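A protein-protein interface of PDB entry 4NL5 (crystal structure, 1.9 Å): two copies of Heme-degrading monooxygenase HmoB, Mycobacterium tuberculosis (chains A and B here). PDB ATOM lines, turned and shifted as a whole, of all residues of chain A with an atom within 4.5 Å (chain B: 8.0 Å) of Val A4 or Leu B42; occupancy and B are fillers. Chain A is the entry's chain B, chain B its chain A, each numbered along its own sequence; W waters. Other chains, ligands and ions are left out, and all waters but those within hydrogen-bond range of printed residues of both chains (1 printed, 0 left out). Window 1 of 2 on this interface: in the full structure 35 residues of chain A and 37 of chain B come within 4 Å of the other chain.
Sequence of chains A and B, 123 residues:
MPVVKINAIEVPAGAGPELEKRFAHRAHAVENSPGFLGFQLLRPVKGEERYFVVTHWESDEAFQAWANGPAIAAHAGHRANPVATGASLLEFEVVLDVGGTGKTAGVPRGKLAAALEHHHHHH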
ATOM      1  N   VAL A   3      -7.501  15.836  -5.927  1.00  0.00           N
ATOM      2  CA  VAL A   3      -6.912  14.516  -5.764  1.00  0.00           C
ATOM      3  C   VAL A   3      -5.612  14.391  -6.532  1.00  0.00           C
ATOM      4  O   VAL A   3      -5.314  15.199  -7.414  1.00  0.00           O
ATOM      5  CB  VAL A   3      -7.878  13.402  -6.216  1.00  0.00           C
ATOM      6  CG1 VAL A   3      -9.132  13.385  -5.316  1.00  0.00           C
ATOM      7  CG2 VAL A   3      -8.266  13.590  -7.659  1.00  0.00           C
ATOM      8  N   VAL A   4      -4.819  13.392  -6.172  1.00  0.00           N
ATOM      9  CA  VAL A   4      -3.584  13.120  -6.891  1.00  0.00           C
ATOM     10  C   VAL A   4      -3.589  11.665  -7.292  1.00  0.00           C
ATOM     11  O   VAL A   4      -3.899  10.786  -6.489  1.00  0.00           O
ATOM     12  CB  VAL A   4      -2.327  13.430  -6.057  1.00  0.00           C
ATOM     13  CG1 VAL A   4      -1.057  12.976  -6.814  1.00  0.00           C
ATOM     14  CG2 VAL A   4      -2.243  14.910  -5.781  1.00  0.00           C
ATOM     15  N   LYS A   5      -3.288  11.426  -8.556  1.00  0.00           N
ATOM     16  CA  LYS A   5      -3.165  10.084  -9.082  1.00  0.00           C
ATOM     17  C   LYS A   5      -1.767   9.931  -9.657  1.00  0.00           C
ATOM     18  O   LYS A   5      -1.414  10.592 -10.631  1.00  0.00           O
ATOM     19  CB  LYS A   5      -4.220   9.829 -10.157  1.00  0.00           C
ATOM     20  CG  LYS A   5      -5.650  10.227  -9.769  1.00  0.00           C
ATOM     21  CD  LYS A   5      -6.292   9.302  -8.744  1.00  0.00           C
ATOM     22  CE  LYS A   5      -7.770   9.676  -8.542  1.00  0.00           C
ATOM     23  NZ  LYS A   5      -8.412   8.852  -7.452  1.00  0.00           N
ATOM     24  N   ILE A   6      -0.967   9.064  -9.057  1.00  0.00           N
ATOM     25  CA  ILE A   6       0.393   8.878  -9.526  1.00  0.00           C
ATOM     26  C   ILE A   6       0.490   7.575 -10.274  1.00  0.00           C
ATOM     27  O   ILE A   6       0.151   6.520  -9.733  1.00  0.00           O
ATOM     28  CB  ILE A   6       1.409   8.873  -8.356  1.00  0.00           C
ATOM     29  CG1 ILE A   6       1.182  10.098  -7.455  1.00  0.00           C
ATOM     30  CG2 ILE A   6       2.839   8.758  -8.912  1.00  0.00           C
ATOM     31  CD1 ILE A   6       2.169  10.226  -6.279  1.00  0.00           C
ATOM     32  N   VAL A  54       2.970  12.258 -11.731  1.00  0.00           N
ATOM     33  CA  VAL A  54       2.127  12.831 -10.686  1.00  0.00           C
ATOM     34  C   VAL A  54       1.073  13.700 -11.336  1.00  0.00           C
ATOM     35  O   VAL A  54       1.374  14.779 -11.823  1.00  0.00           O
ATOM     36  CB  VAL A  54       2.955  13.673  -9.663  1.00  0.00           C
ATOM     37  CG1 VAL A  54       2.063  14.197  -8.500  1.00  0.00           C
ATOM     38  CG2 VAL A  54       4.086  12.833  -9.095  1.00  0.00           C
ATOM     39  N   THR A  55      -0.165  13.225 -11.361  1.00  0.00           N
ATOM     40  CA  THR A  55      -1.225  13.987 -12.013  1.00  0.00           C
ATOM     41  C   THR A  55      -2.205  14.541 -10.984  1.00  0.00           C
ATOM     42  O   THR A  55      -2.497  13.897  -9.977  1.00  0.00           O
ATOM     43  CB  THR A  55      -1.970  13.141 -13.046  1.00  0.00           C
ATOM     44  OG1 THR A  55      -2.750  12.134 -12.388  1.00  0.00           O
ATOM     45  CG2 THR A  55      -0.973  12.457 -13.968  1.00  0.00           C
ATOM     46  N   HIS A  56      -2.684  15.754 -11.241  1.00  0.00           N
ATOM     47  CA  HIS A  56      -3.526  16.485 -10.303  1.00  0.00           C
ATOM     48  C   HIS A  56      -4.903  16.741 -10.914  1.00  0.00           C
ATOM     49  O   HIS A  56      -4.989  17.136 -12.068  1.00  0.00           O
ATOM     50  CB  HIS A  56      -2.867  17.814  -9.928  1.00  0.00           C
ATOM     51  CG  HIS A  56      -1.450  17.675  -9.455  1.00  0.00           C
ATOM     52  ND1 HIS A  56      -1.111  17.649  -8.119  1.00  0.00           N
ATOM     53  CD2 HIS A  56      -0.286  17.574 -10.142  1.00  0.00           C
ATOM     54  CE1 HIS A  56       0.202  17.530  -8.002  1.00  0.00           C
ATOM     55  NE2 HIS A  56       0.727  17.483  -9.216  1.00  0.00           N
ATOM     56  N   LEU A  90      -1.213   4.931  -7.968  1.00  0.00           N
ATOM     57  CA  LEU A  90      -1.271   5.294  -6.546  1.00  0.00           C
ATOM     58  C   LEU A  90      -2.209   6.477  -6.384  1.00  0.00           C
ATOM     59  O   LEU A  90      -2.011   7.521  -7.006  1.00  0.00           O
ATOM     60  CB  LEU A  90       0.121   5.646  -6.012  1.00  0.00           C
ATOM     61  CG  LEU A  90       1.300   4.783  -6.458  1.00  0.00           C
ATOM     62  CD1 LEU A  90       2.626   5.296  -5.825  1.00  0.00           C
ATOM     63  CD2 LEU A  90       1.050   3.325  -6.119  1.00  0.00           C
ATOM     64  N   GLU A  91      -3.253   6.315  -5.584  1.00  0.00           N
ATOM     65  CA  GLU A  91      -4.309   7.318  -5.530  1.00  0.00           C
ATOM     66  C   GLU A  91      -4.392   7.981  -4.158  1.00  0.00           C
ATOM     67  O   GLU A  91      -4.427   7.296  -3.133  1.00  0.00           O
ATOM     68  CB  GLU A  91      -5.667   6.684  -5.903  1.00  0.00           C
ATOM     69  CG  GLU A  91      -5.636   5.907  -7.231  1.00  0.00           C
ATOM     70  CD  GLU A  91      -7.000   5.349  -7.661  1.00  0.00           C
ATOM     71  OE1 GLU A  91      -7.989   6.114  -7.724  1.00  0.00           O
ATOM     72  OE2 GLU A  91      -7.080   4.133  -7.937  1.00  0.00           O
ATOM     73  N   PHE A  92      -4.454   9.313  -4.168  1.00  0.00           N
ATOM     74  CA  PHE A  92      -4.426  10.137  -2.961  1.00  0.00           C
ATOM     75  C   PHE A  92      -5.480  11.241  -2.982  1.00  0.00           C
ATOM     76  O   PHE A  92      -5.928  11.679  -4.050  1.00  0.00           O
ATOM     77  CB  PHE A  92      -3.048  10.811  -2.783  1.00  0.00           C
ATOM     78  CG  PHE A  92      -1.904   9.854  -2.662  1.00  0.00           C
ATOM     79  CD1 PHE A  92      -1.462   9.426  -1.415  1.00  0.00           C
ATOM     80  CD2 PHE A  92      -1.233   9.413  -3.796  1.00  0.00           C
ATOM     81  CE1 PHE A  92      -0.398   8.552  -1.293  1.00  0.00           C
ATOM     82  CE2 PHE A  92      -0.149   8.542  -3.685  1.00  0.00           C
ATOM     83  CZ  PHE A  92       0.268   8.113  -2.442  1.00  0.00           C
ATOM     84  N   GLU A  93      -5.850  11.705  -1.795  1.00  0.00           N
ATOM     85  CA  GLU A  93      -6.594  12.947  -1.629  1.00  0.00           C
ATOM     86  C   GLU A  93      -5.650  14.001  -1.074  1.00  0.00           C
ATOM     87  O   GLU A  93      -4.834  13.700  -0.200  1.00  0.00           O
ATOM     88  CB  GLU A  93      -7.796  12.754  -0.691  1.00  0.00           C
ATOM     89  CG  GLU A  93      -8.932  11.990  -1.353  1.00  0.00           C
ATOM     90  CD  GLU A  93      -9.927  11.405  -0.369  1.00  0.00           C
ATOM     91  OE1 GLU A  93      -9.737  11.550   0.866  1.00  0.00           O
ATOM     92  OE2 GLU A  93     -10.907  10.792  -0.842  1.00  0.00           O
ATOM     93  N   VAL A  94      -5.757  15.232  -1.566  1.00  0.00           N
ATOM     94  CA  VAL A  94      -4.916  16.305  -1.053  1.00  0.00           C
ATOM     95  C   VAL A  94      -5.474  16.809   0.281  1.00  0.00           C
ATOM     96  O   VAL A  94      -6.611  17.269   0.350  1.00  0.00           O
ATOM     97  CB  VAL A  94      -4.797  17.465  -2.045  1.00  0.00           C
ATOM     98  CG1 VAL A  94      -3.889  18.549  -1.470  1.00  0.00           C
ATOM     99  CG2 VAL A  94      -4.236  16.956  -3.369  1.00  0.00           C
ATOM    100  N   ILE B   6       9.869  13.158  -1.434  1.00  0.00           N
ATOM    101  CA  ILE B   6       8.641  12.661  -0.831  1.00  0.00           C
ATOM    102  C   ILE B   6       8.971  11.870   0.416  1.00  0.00           C
ATOM    103  O   ILE B   6       9.644  10.849   0.317  1.00  0.00           O
ATOM    104  CB  ILE B   6       7.869  11.739  -1.796  1.00  0.00           C
ATOM    105  CG1 ILE B   6       7.573  12.458  -3.116  1.00  0.00           C
ATOM    106  CG2 ILE B   6       6.574  11.254  -1.138  1.00  0.00           C
ATOM    107  CD1 ILE B   6       6.785  11.603  -4.100  1.00  0.00           C
ATOM    108  N   ASN B   7       8.476  12.308   1.573  1.00  0.00           N
ATOM    109  CA  ASN B   7       8.562  11.487   2.765  1.00  0.00           C
ATOM    110  C   ASN B   7       7.321  10.622   2.823  1.00  0.00           C
ATOM    111  O   ASN B   7       6.202  11.129   2.975  1.00  0.00           O
ATOM    112  CB  ASN B   7       8.701  12.333   4.027  1.00  0.00           C
ATOM    113  CG  ASN B   7       9.414  11.593   5.144  1.00  0.00           C
ATOM    114  OD1 ASN B   7      10.346  10.834   4.890  1.00  0.00           O
ATOM    115  ND2 ASN B   7       8.995  11.828   6.385  1.00  0.00           N
ATOM    116  N   ILE B   9       5.196   8.225   4.797  1.00  0.00           N
ATOM    117  CA  ILE B   9       5.017   7.957   6.227  1.00  0.00           C
ATOM    118  C   ILE B   9       4.075   6.792   6.462  1.00  0.00           C
ATOM    119  O   ILE B   9       2.987   6.749   5.900  1.00  0.00           O
ATOM    120  CB  ILE B   9       4.456   9.185   6.940  1.00  0.00           C
ATOM    121  CG1 ILE B   9       5.443  10.340   6.887  1.00  0.00           C
ATOM    122  CG2 ILE B   9       4.119   8.864   8.395  1.00  0.00           C
ATOM    123  CD1 ILE B   9       4.876  11.595   7.491  1.00  0.00           C
ATOM    124  N   LEU B  19      -2.405  12.584  12.521  1.00  0.00           N
ATOM    125  CA  LEU B  19      -1.245  12.960  11.712  1.00  0.00           C
ATOM    126  C   LEU B  19      -1.545  14.225  10.912  1.00  0.00           C
ATOM    127  O   LEU B  19      -0.762  15.173  10.891  1.00  0.00           O
ATOM    128  CB  LEU B  19      -0.840  11.825  10.770  1.00  0.00           C
ATOM    129  CG  LEU B  19       0.404  12.135   9.940  1.00  0.00           C
ATOM    130  CD1 LEU B  19       1.659  11.730  10.699  1.00  0.00           C
ATOM    131  CD2 LEU B  19       0.343  11.450   8.599  1.00  0.00           C
ATOM    132  N   GLU B  20      -2.704  14.236  10.269  1.00  0.00           N
ATOM    133  CA  GLU B  20      -3.115  15.363   9.452  1.00  0.00           C
ATOM    134  C   GLU B  20      -3.215  16.624  10.295  1.00  0.00           C
ATOM    135  O   GLU B  20      -2.801  17.705   9.878  1.00  0.00           O
ATOM    136  CB  GLU B  20      -4.458  15.057   8.782  1.00  0.00           C
ATOM    137  CG  GLU B  20      -4.370  13.960   7.738  1.00  0.00           C
ATOM    138  CD  GLU B  20      -5.724  13.575   7.180  1.00  0.00           C
ATOM    139  OE1 GLU B  20      -6.699  14.333   7.387  1.00  0.00           O
ATOM    140  OE2 GLU B  20      -5.806  12.526   6.506  1.00  0.00           O
ATOM    141  N   PHE B  23       0.333  17.949  11.062  1.00  0.00           N
ATOM    142  CA  PHE B  23       0.863  18.618   9.867  1.00  0.00           C
ATOM    143  C   PHE B  23       0.236  19.998   9.665  1.00  0.00           C
ATOM    144  O   PHE B  23       0.927  20.958   9.338  1.00  0.00           O
ATOM    145  CB  PHE B  23       0.648  17.763   8.614  1.00  0.00           C
ATOM    146  CG  PHE B  23       1.802  16.855   8.300  1.00  0.00           C
ATOM    147  CD1 PHE B  23       2.848  17.288   7.498  1.00  0.00           C
ATOM    148  CD2 PHE B  23       1.854  15.577   8.834  1.00  0.00           C
ATOM    149  CE1 PHE B  23       3.921  16.451   7.220  1.00  0.00           C
ATOM    150  CE2 PHE B  23       2.917  14.735   8.563  1.00  0.00           C
ATOM    151  CZ  PHE B  23       3.953  15.174   7.755  1.00  0.00           C
ATOM    152  N   PHE B  39       4.767  22.284  -0.263  1.00  0.00           N
ATOM    153  CA  PHE B  39       4.518  20.874  -0.063  1.00  0.00           C
ATOM    154  C   PHE B  39       3.038  20.562  -0.050  1.00  0.00           C
ATOM    155  O   PHE B  39       2.202  21.437   0.141  1.00  0.00           O
ATOM    156  CB  PHE B  39       5.171  20.384   1.237  1.00  0.00           C
ATOM    157  CG  PHE B  39       4.311  20.553   2.481  1.00  0.00           C
ATOM    158  CD1 PHE B  39       3.640  19.471   3.030  1.00  0.00           C
ATOM    159  CD2 PHE B  39       4.227  21.779   3.124  1.00  0.00           C
ATOM    160  CE1 PHE B  39       2.873  19.619   4.172  1.00  0.00           C
ATOM    161  CE2 PHE B  39       3.461  21.934   4.261  1.00  0.00           C
ATOM    162  CZ  PHE B  39       2.783  20.848   4.789  1.00  0.00           C
ATOM    163  N   GLN B  40       2.741  19.301  -0.308  1.00  0.00           N
ATOM    164  CA  GLN B  40       1.392  18.773  -0.162  1.00  0.00           C
ATOM    165  C   GLN B  40       1.449  17.578   0.751  1.00  0.00           C
ATOM    166  O   GLN B  40       2.406  16.798   0.703  1.00  0.00           O
ATOM    167  CB  GLN B  40       0.791  18.366  -1.512  1.00  0.00           C
ATOM    168  CG  GLN B  40       0.645  19.515  -2.514  1.00  0.00           C
ATOM    169  CD  GLN B  40       1.944  19.847  -3.211  1.00  0.00           C
ATOM    170  OE1 GLN B  40       2.708  18.953  -3.587  1.00  0.00           O
ATOM    171  NE2 GLN B  40       2.204  21.139  -3.393  1.00  0.00           N
ATOM    172  N   LEU B  41       0.424  17.446   1.583  1.00  0.00           N
ATOM    173  CA  LEU B  41       0.213  16.243   2.359  1.00  0.00           C
ATOM    174  C   LEU B  41      -0.857  15.414   1.664  1.00  0.00           C
ATOM    175  O   LEU B  41      -1.993  15.860   1.523  1.00  0.00           O
ATOM    176  CB  LEU B  41      -0.216  16.574   3.790  1.00  0.00           C
ATOM    177  CG  LEU B  41      -0.555  15.336   4.627  1.00  0.00           C
ATOM    178  CD1 LEU B  41       0.686  14.474   4.835  1.00  0.00           C
ATOM    179  CD2 LEU B  41      -1.161  15.726   5.973  1.00  0.00           C
ATOM    180  N   LEU B  42      -0.491  14.209   1.249  1.00  0.00           N
ATOM    181  CA  LEU B  42      -1.394  13.349   0.484  1.00  0.00           C
ATOM    182  C   LEU B  42      -1.885  12.158   1.297  1.00  0.00           C
ATOM    183  O   LEU B  42      -1.083  11.334   1.729  1.00  0.00           O
ATOM    184  CB  LEU B  42      -0.696  12.827  -0.767  1.00  0.00           C
ATOM    185  CG  LEU B  42      -0.168  13.897  -1.723  1.00  0.00           C
ATOM    186  CD1 LEU B  42       0.334  13.283  -3.047  1.00  0.00           C
ATOM    187  CD2 LEU B  42      -1.240  14.948  -1.962  1.00  0.00           C
ATOM    188  N   ARG B  43      -3.204  12.066   1.454  1.00  0.00           N
ATOM    189  CA  ARG B  43      -3.854  10.946   2.133  1.00  0.00           C
ATOM    190  C   ARG B  43      -4.086   9.795   1.171  1.00  0.00           C
ATOM    191  O   ARG B  43      -4.726   9.983   0.140  1.00  0.00           O
ATOM    192  CB  ARG B  43      -5.202  11.377   2.706  1.00  0.00           C
ATOM    193  CG  ARG B  43      -5.983  10.246   3.359  1.00  0.00           C
ATOM    194  CD  ARG B  43      -7.434  10.652   3.545  1.00  0.00           C
ATOM    195  NE  ARG B  43      -7.588  11.830   4.389  1.00  0.00           N
ATOM    196  CZ  ARG B  43      -8.242  12.925   4.018  1.00  0.00           C
ATOM    197  NH1 ARG B  43      -8.778  12.994   2.806  1.00  0.00           N
ATOM    198  NH2 ARG B  43      -8.339  13.962   4.841  1.00  0.00           N
ATOM    199  N   PRO B  44      -3.591   8.600   1.507  1.00  0.00           N
ATOM    200  CA  PRO B  44      -3.747   7.452   0.607  1.00  0.00           C
ATOM    201  C   PRO B  44      -5.192   6.969   0.509  1.00  0.00           C
ATOM    202  O   PRO B  44      -5.907   6.952   1.514  1.00  0.00           O
ATOM    203  CB  PRO B  44      -2.857   6.383   1.247  1.00  0.00           C
ATOM    204  CG  PRO B  44      -2.831   6.746   2.699  1.00  0.00           C
ATOM    205  CD  PRO B  44      -2.820   8.256   2.718  1.00  0.00           C
ATOM    206  N   VAL B  45      -5.607   6.584  -0.695  1.00  0.00           N
ATOM    207  CA  VAL B  45      -6.982   6.134  -0.934  1.00  0.00           C
ATOM    208  C   VAL B  45      -6.982   4.759  -1.608  1.00  0.00           C
ATOM    209  O   VAL B  45      -7.838   3.919  -1.326  1.00  0.00           O
ATOM    210  CB  VAL B  45      -7.761   7.160  -1.792  1.00  0.00           C
ATOM    211  CG1 VAL B  45      -8.969   6.514  -2.462  1.00  0.00           C
ATOM    212  CG2 VAL B  45      -8.207   8.313  -0.910  1.00  0.00           C
ATOM    213  N   LYS B  46      -6.023   4.525  -2.498  1.00  0.00           N
ATOM    214  CA  LYS B  46      -5.901   3.220  -3.144  1.00  0.00           C
ATOM    215  C   LYS B  46      -4.478   3.013  -3.679  1.00  0.00           C
ATOM    216  O   LYS B  46      -3.845   3.952  -4.141  1.00  0.00           O
ATOM    217  CB  LYS B  46      -6.919   3.100  -4.274  1.00  0.00           C
ATOM    218  CG  LYS B  46      -7.127   1.689  -4.815  1.00  0.00           C
ATOM    219  CD  LYS B  46      -8.311   1.663  -5.770  1.00  0.00           C
ATOM    220  CE  LYS B  46      -8.587   0.263  -6.279  1.00  0.00           C
ATOM    221  NZ  LYS B  46      -7.443  -0.243  -7.082  1.00  0.00           N
ATOM    222  N   GLU B  48      -1.697   2.602  -2.177  1.00  0.00           N
ATOM    223  CA  GLU B  48      -0.670   2.925  -1.171  1.00  0.00           C
ATOM    224  C   GLU B  48      -1.346   2.959   0.186  1.00  0.00           C
ATOM    225  O   GLU B  48      -2.530   3.280   0.274  1.00  0.00           O
ATOM    226  CB  GLU B  48       0.001   4.280  -1.446  1.00  0.00           C
ATOM    227  CG  GLU B  48       1.381   4.239  -2.106  1.00  0.00           C
ATOM    228  CD  GLU B  48       2.495   3.733  -1.198  1.00  0.00           C
ATOM    229  OE1 GLU B  48       3.546   3.322  -1.737  1.00  0.00           O
ATOM    230  OE2 GLU B  48       2.342   3.747   0.043  1.00  0.00           O
ATOM    231  N   GLU B  49      -0.604   2.638   1.239  1.00  0.00           N
ATOM    232  CA  GLU B  49      -1.135   2.760   2.584  1.00  0.00           C
ATOM    233  C   GLU B  49      -0.412   3.870   3.337  1.00  0.00           C
ATOM    234  O   GLU B  49      -0.787   4.216   4.457  1.00  0.00           O
ATOM    235  CB  GLU B  49      -1.006   1.433   3.342  1.00  0.00           C
ATOM    236  CG  GLU B  49      -1.700   0.247   2.674  1.00  0.00           C
ATOM    237  CD  GLU B  49      -1.459  -1.063   3.413  1.00  0.00           C
ATOM    238  OE1 GLU B  49      -1.191  -1.021   4.633  1.00  0.00           O
ATOM    239  OE2 GLU B  49      -1.521  -2.137   2.777  1.00  0.00           O
ATOM    240  N   ARG B  50       0.632   4.424   2.720  1.00  0.00           N
ATOM    241  CA  ARG B  50       1.412   5.466   3.359  1.00  0.00           C
ATOM    242  C   ARG B  50       0.909   6.845   2.975  1.00  0.00           C
ATOM    243  O   ARG B  50       0.419   7.049   1.862  1.00  0.00           O
ATOM    244  CB  ARG B  50       2.897   5.333   2.977  1.00  0.00           C
ATOM    245  CG  ARG B  50       3.539   4.019   3.415  1.00  0.00           C
ATOM    246  CD  ARG B  50       4.956   3.890   2.867  1.00  0.00           C
ATOM    247  NE  ARG B  50       4.959   3.842   1.404  1.00  0.00           N
ATOM    248  CZ  ARG B  50       6.051   3.713   0.657  1.00  0.00           C
ATOM    249  NH1 ARG B  50       7.239   3.629   1.239  1.00  0.00           N
ATOM    250  NH2 ARG B  50       5.956   3.671  -0.670  1.00  0.00           N
ATOM    251  N   TYR B  51       1.041   7.796   3.890  1.00  0.00           N
ATOM    252  CA  TYR B  51       0.869   9.199   3.540  1.00  0.00           C
ATOM    253  C   TYR B  51       2.075   9.657   2.729  1.00  0.00           C
ATOM    254  O   TYR B  51       3.201   9.290   3.038  1.00  0.00           O
ATOM    255  CB  TYR B  51       0.703  10.063   4.796  1.00  0.00           C
ATOM    256  CG  TYR B  51      -0.708  10.128   5.337  1.00  0.00           C
ATOM    257  CD1 TYR B  51      -1.478  11.276   5.175  1.00  0.00           C
ATOM    258  CD2 TYR B  51      -1.269   9.055   6.025  1.00  0.00           C
ATOM    259  CE1 TYR B  51      -2.765  11.352   5.672  1.00  0.00           C
ATOM    260  CE2 TYR B  51      -2.568   9.121   6.524  1.00  0.00           C
ATOM    261  CZ  TYR B  51      -3.301  10.271   6.347  1.00  0.00           C
ATOM    262  OH  TYR B  51      -4.567  10.350   6.839  1.00  0.00           O
ATOM    263  N   PHE B  52       1.846  10.430   1.672  1.00  0.00           N
ATOM    264  CA  PHE B  52       2.965  11.014   0.936  1.00  0.00           C
ATOM    265  C   PHE B  52       3.077  12.495   1.275  1.00  0.00           C
ATOM    266  O   PHE B  52       2.136  13.270   1.046  1.00  0.00           O
ATOM    267  CB  PHE B  52       2.804  10.866  -0.590  1.00  0.00           C
ATOM    268  CG  PHE B  52       3.230   9.529  -1.154  1.00  0.00           C
ATOM    269  CD1 PHE B  52       3.439   8.425  -0.338  1.00  0.00           C
ATOM    270  CD2 PHE B  52       3.420   9.387  -2.535  1.00  0.00           C
ATOM    271  CE1 PHE B  52       3.818   7.195  -0.891  1.00  0.00           C
ATOM    272  CE2 PHE B  52       3.806   8.176  -3.088  1.00  0.00           C
ATOM    273  CZ  PHE B  52       4.006   7.071  -2.258  1.00  0.00           C
ATOM    274  N   VAL B  53       4.229  12.888   1.807  1.00  0.00           N
ATOM    275  CA  VAL B  53       4.505  14.286   2.052  1.00  0.00           C
ATOM    276  C   VAL B  53       5.380  14.777   0.907  1.00  0.00           C
ATOM    277  O   VAL B  53       6.572  14.509   0.878  1.00  0.00           O
ATOM    278  CB  VAL B  53       5.191  14.486   3.411  1.00  0.00           C
ATOM    279  CG1 VAL B  53       5.474  15.956   3.655  1.00  0.00           C
ATOM    280  CG2 VAL B  53       4.293  13.909   4.525  1.00  0.00           C
ATOM    281  N   VAL B  54       4.766  15.456  -0.055  1.00  0.00           N
ATOM    282  CA  VAL B  54       5.444  15.796  -1.303  1.00  0.00           C
ATOM    283  C   VAL B  54       6.051  17.180  -1.201  1.00  0.00           C
ATOM    284  O   VAL B  54       5.329  18.166  -1.238  1.00  0.00           O
ATOM    285  CB  VAL B  54       4.477  15.748  -2.521  1.00  0.00           C
ATOM    286  CG1 VAL B  54       5.250  16.004  -3.832  1.00  0.00           C
ATOM    287  CG2 VAL B  54       3.760  14.408  -2.592  1.00  0.00           C
HETATM  288  O   HOH W   1      -5.249   2.254  -7.738  1.00  0.00           O
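The side-chain carboxylate of Glu A93 lies within salt-bridge range of the guanidinium group of Arg B43.
The backbone NH (N) of Val B45 sits at hydrogen-bond distance from the backbone carbonyl oxygen (O) of Glu A91 (2.8 Å).
O of Lys B46 lies within hydrogen-bond range of N of Glu A91 (2.8 Å).
The guanidinium group (NE) of Arg B43 lies within salt-bridge range of the side-chain carboxylate (OE2) of Glu B20 (2.9 Å).
The backbone NH of Leu B42 is in hydrogen-bond range of the backbone carbonyl oxygen of Phe B52.
OE1 of Glu B48 is in salt-bridge range of NH2 of Arg B50, 2.7 Å away.
N of Phe A92 lies within hydrogen-bond range of O of Val A4 (2.8 Å).
OE1 of Glu A91 lies within salt-bridge range of NZ of Lys A5 (2.8 Å).
The backbone carbonyl oxygen (O) of Ile A6 sits at hydrogen-bond distance from the backbone NH (N) of Leu A90, at 2.7 Å.
Among the printed residues, merely in contact across the chains: Phe A92 with Arg B43 (3.1 Å), Phe A92 with Phe B52 (3.4 Å), Glu A93 with Leu B42 (3.5 Å), Phe A92 with Leu B42 (3.5 Å), Glu A93 with Val B45 (3.6 Å), Phe A92 with Arg B50 (3.6 Å), Phe A92 with Pro B44 (3.6 Å), Glu A91 with Pro B44 (3.7 Å), Leu A90 with Lys B46 (3.8 Å), Val A94 with Leu B41 (3.8 Å), Val A94 with Leu B42 (3.9 Å), Val A4 with Leu B42 (3.9 Å), Glu A93 with Leu B41 (3.96 Å) and Phe A92 with Glu B48 (3.97 Å).
Leu B42 touches just these residues of chain A: Val A4, Phe A92, Glu A93 and Val A94.
Printed residues of chain A within 4 Å of Lys B46: Leu A90 and Glu A91.
Of the printed residues of chain B, Val A94 touches Leu B41 (3.8 Å) and Leu B42 (3.9 Å).
Of the printed residues of chain A, Glu B48 touches Phe A92 (3.97 Å).
Of the printed residues of chain A, Arg B50 touches Phe A92.
Glu B49 touches none of the printed residues of chain A.
The nearest residue of chain B that does not touch Val A4 is Gln B40 (6.3 Å).
Printed residues of chain A that touch a printed residue of chain B: Val A4, Leu A90, Glu A91, Phe A92, Glu A93 and Val A94.
Hydrophobic or aromatic side chains of chain A within 4 Å of the printed part of chain B: Val A4, Phe A92 and Val A94.
Printed residues of chain B that touch a printed residue of chain A: Leu B41, Leu B42, Arg B43, Pro B44, Val B45, Lys B46, Glu B48, Arg B50 and Phe B52.
Among the printed residues, 17 pairs touch across the chains.
Positions printed for both chains: 6 and 54.
Of the 17 pairs that touch across the chains among the printed residues, none has its exchanged pair printed and touching as well.
Water W1 lies within hydrogen-bond range of OE2 of Glu A91 (2.6 Å) and NZ of Lys B46 (3.4 Å).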
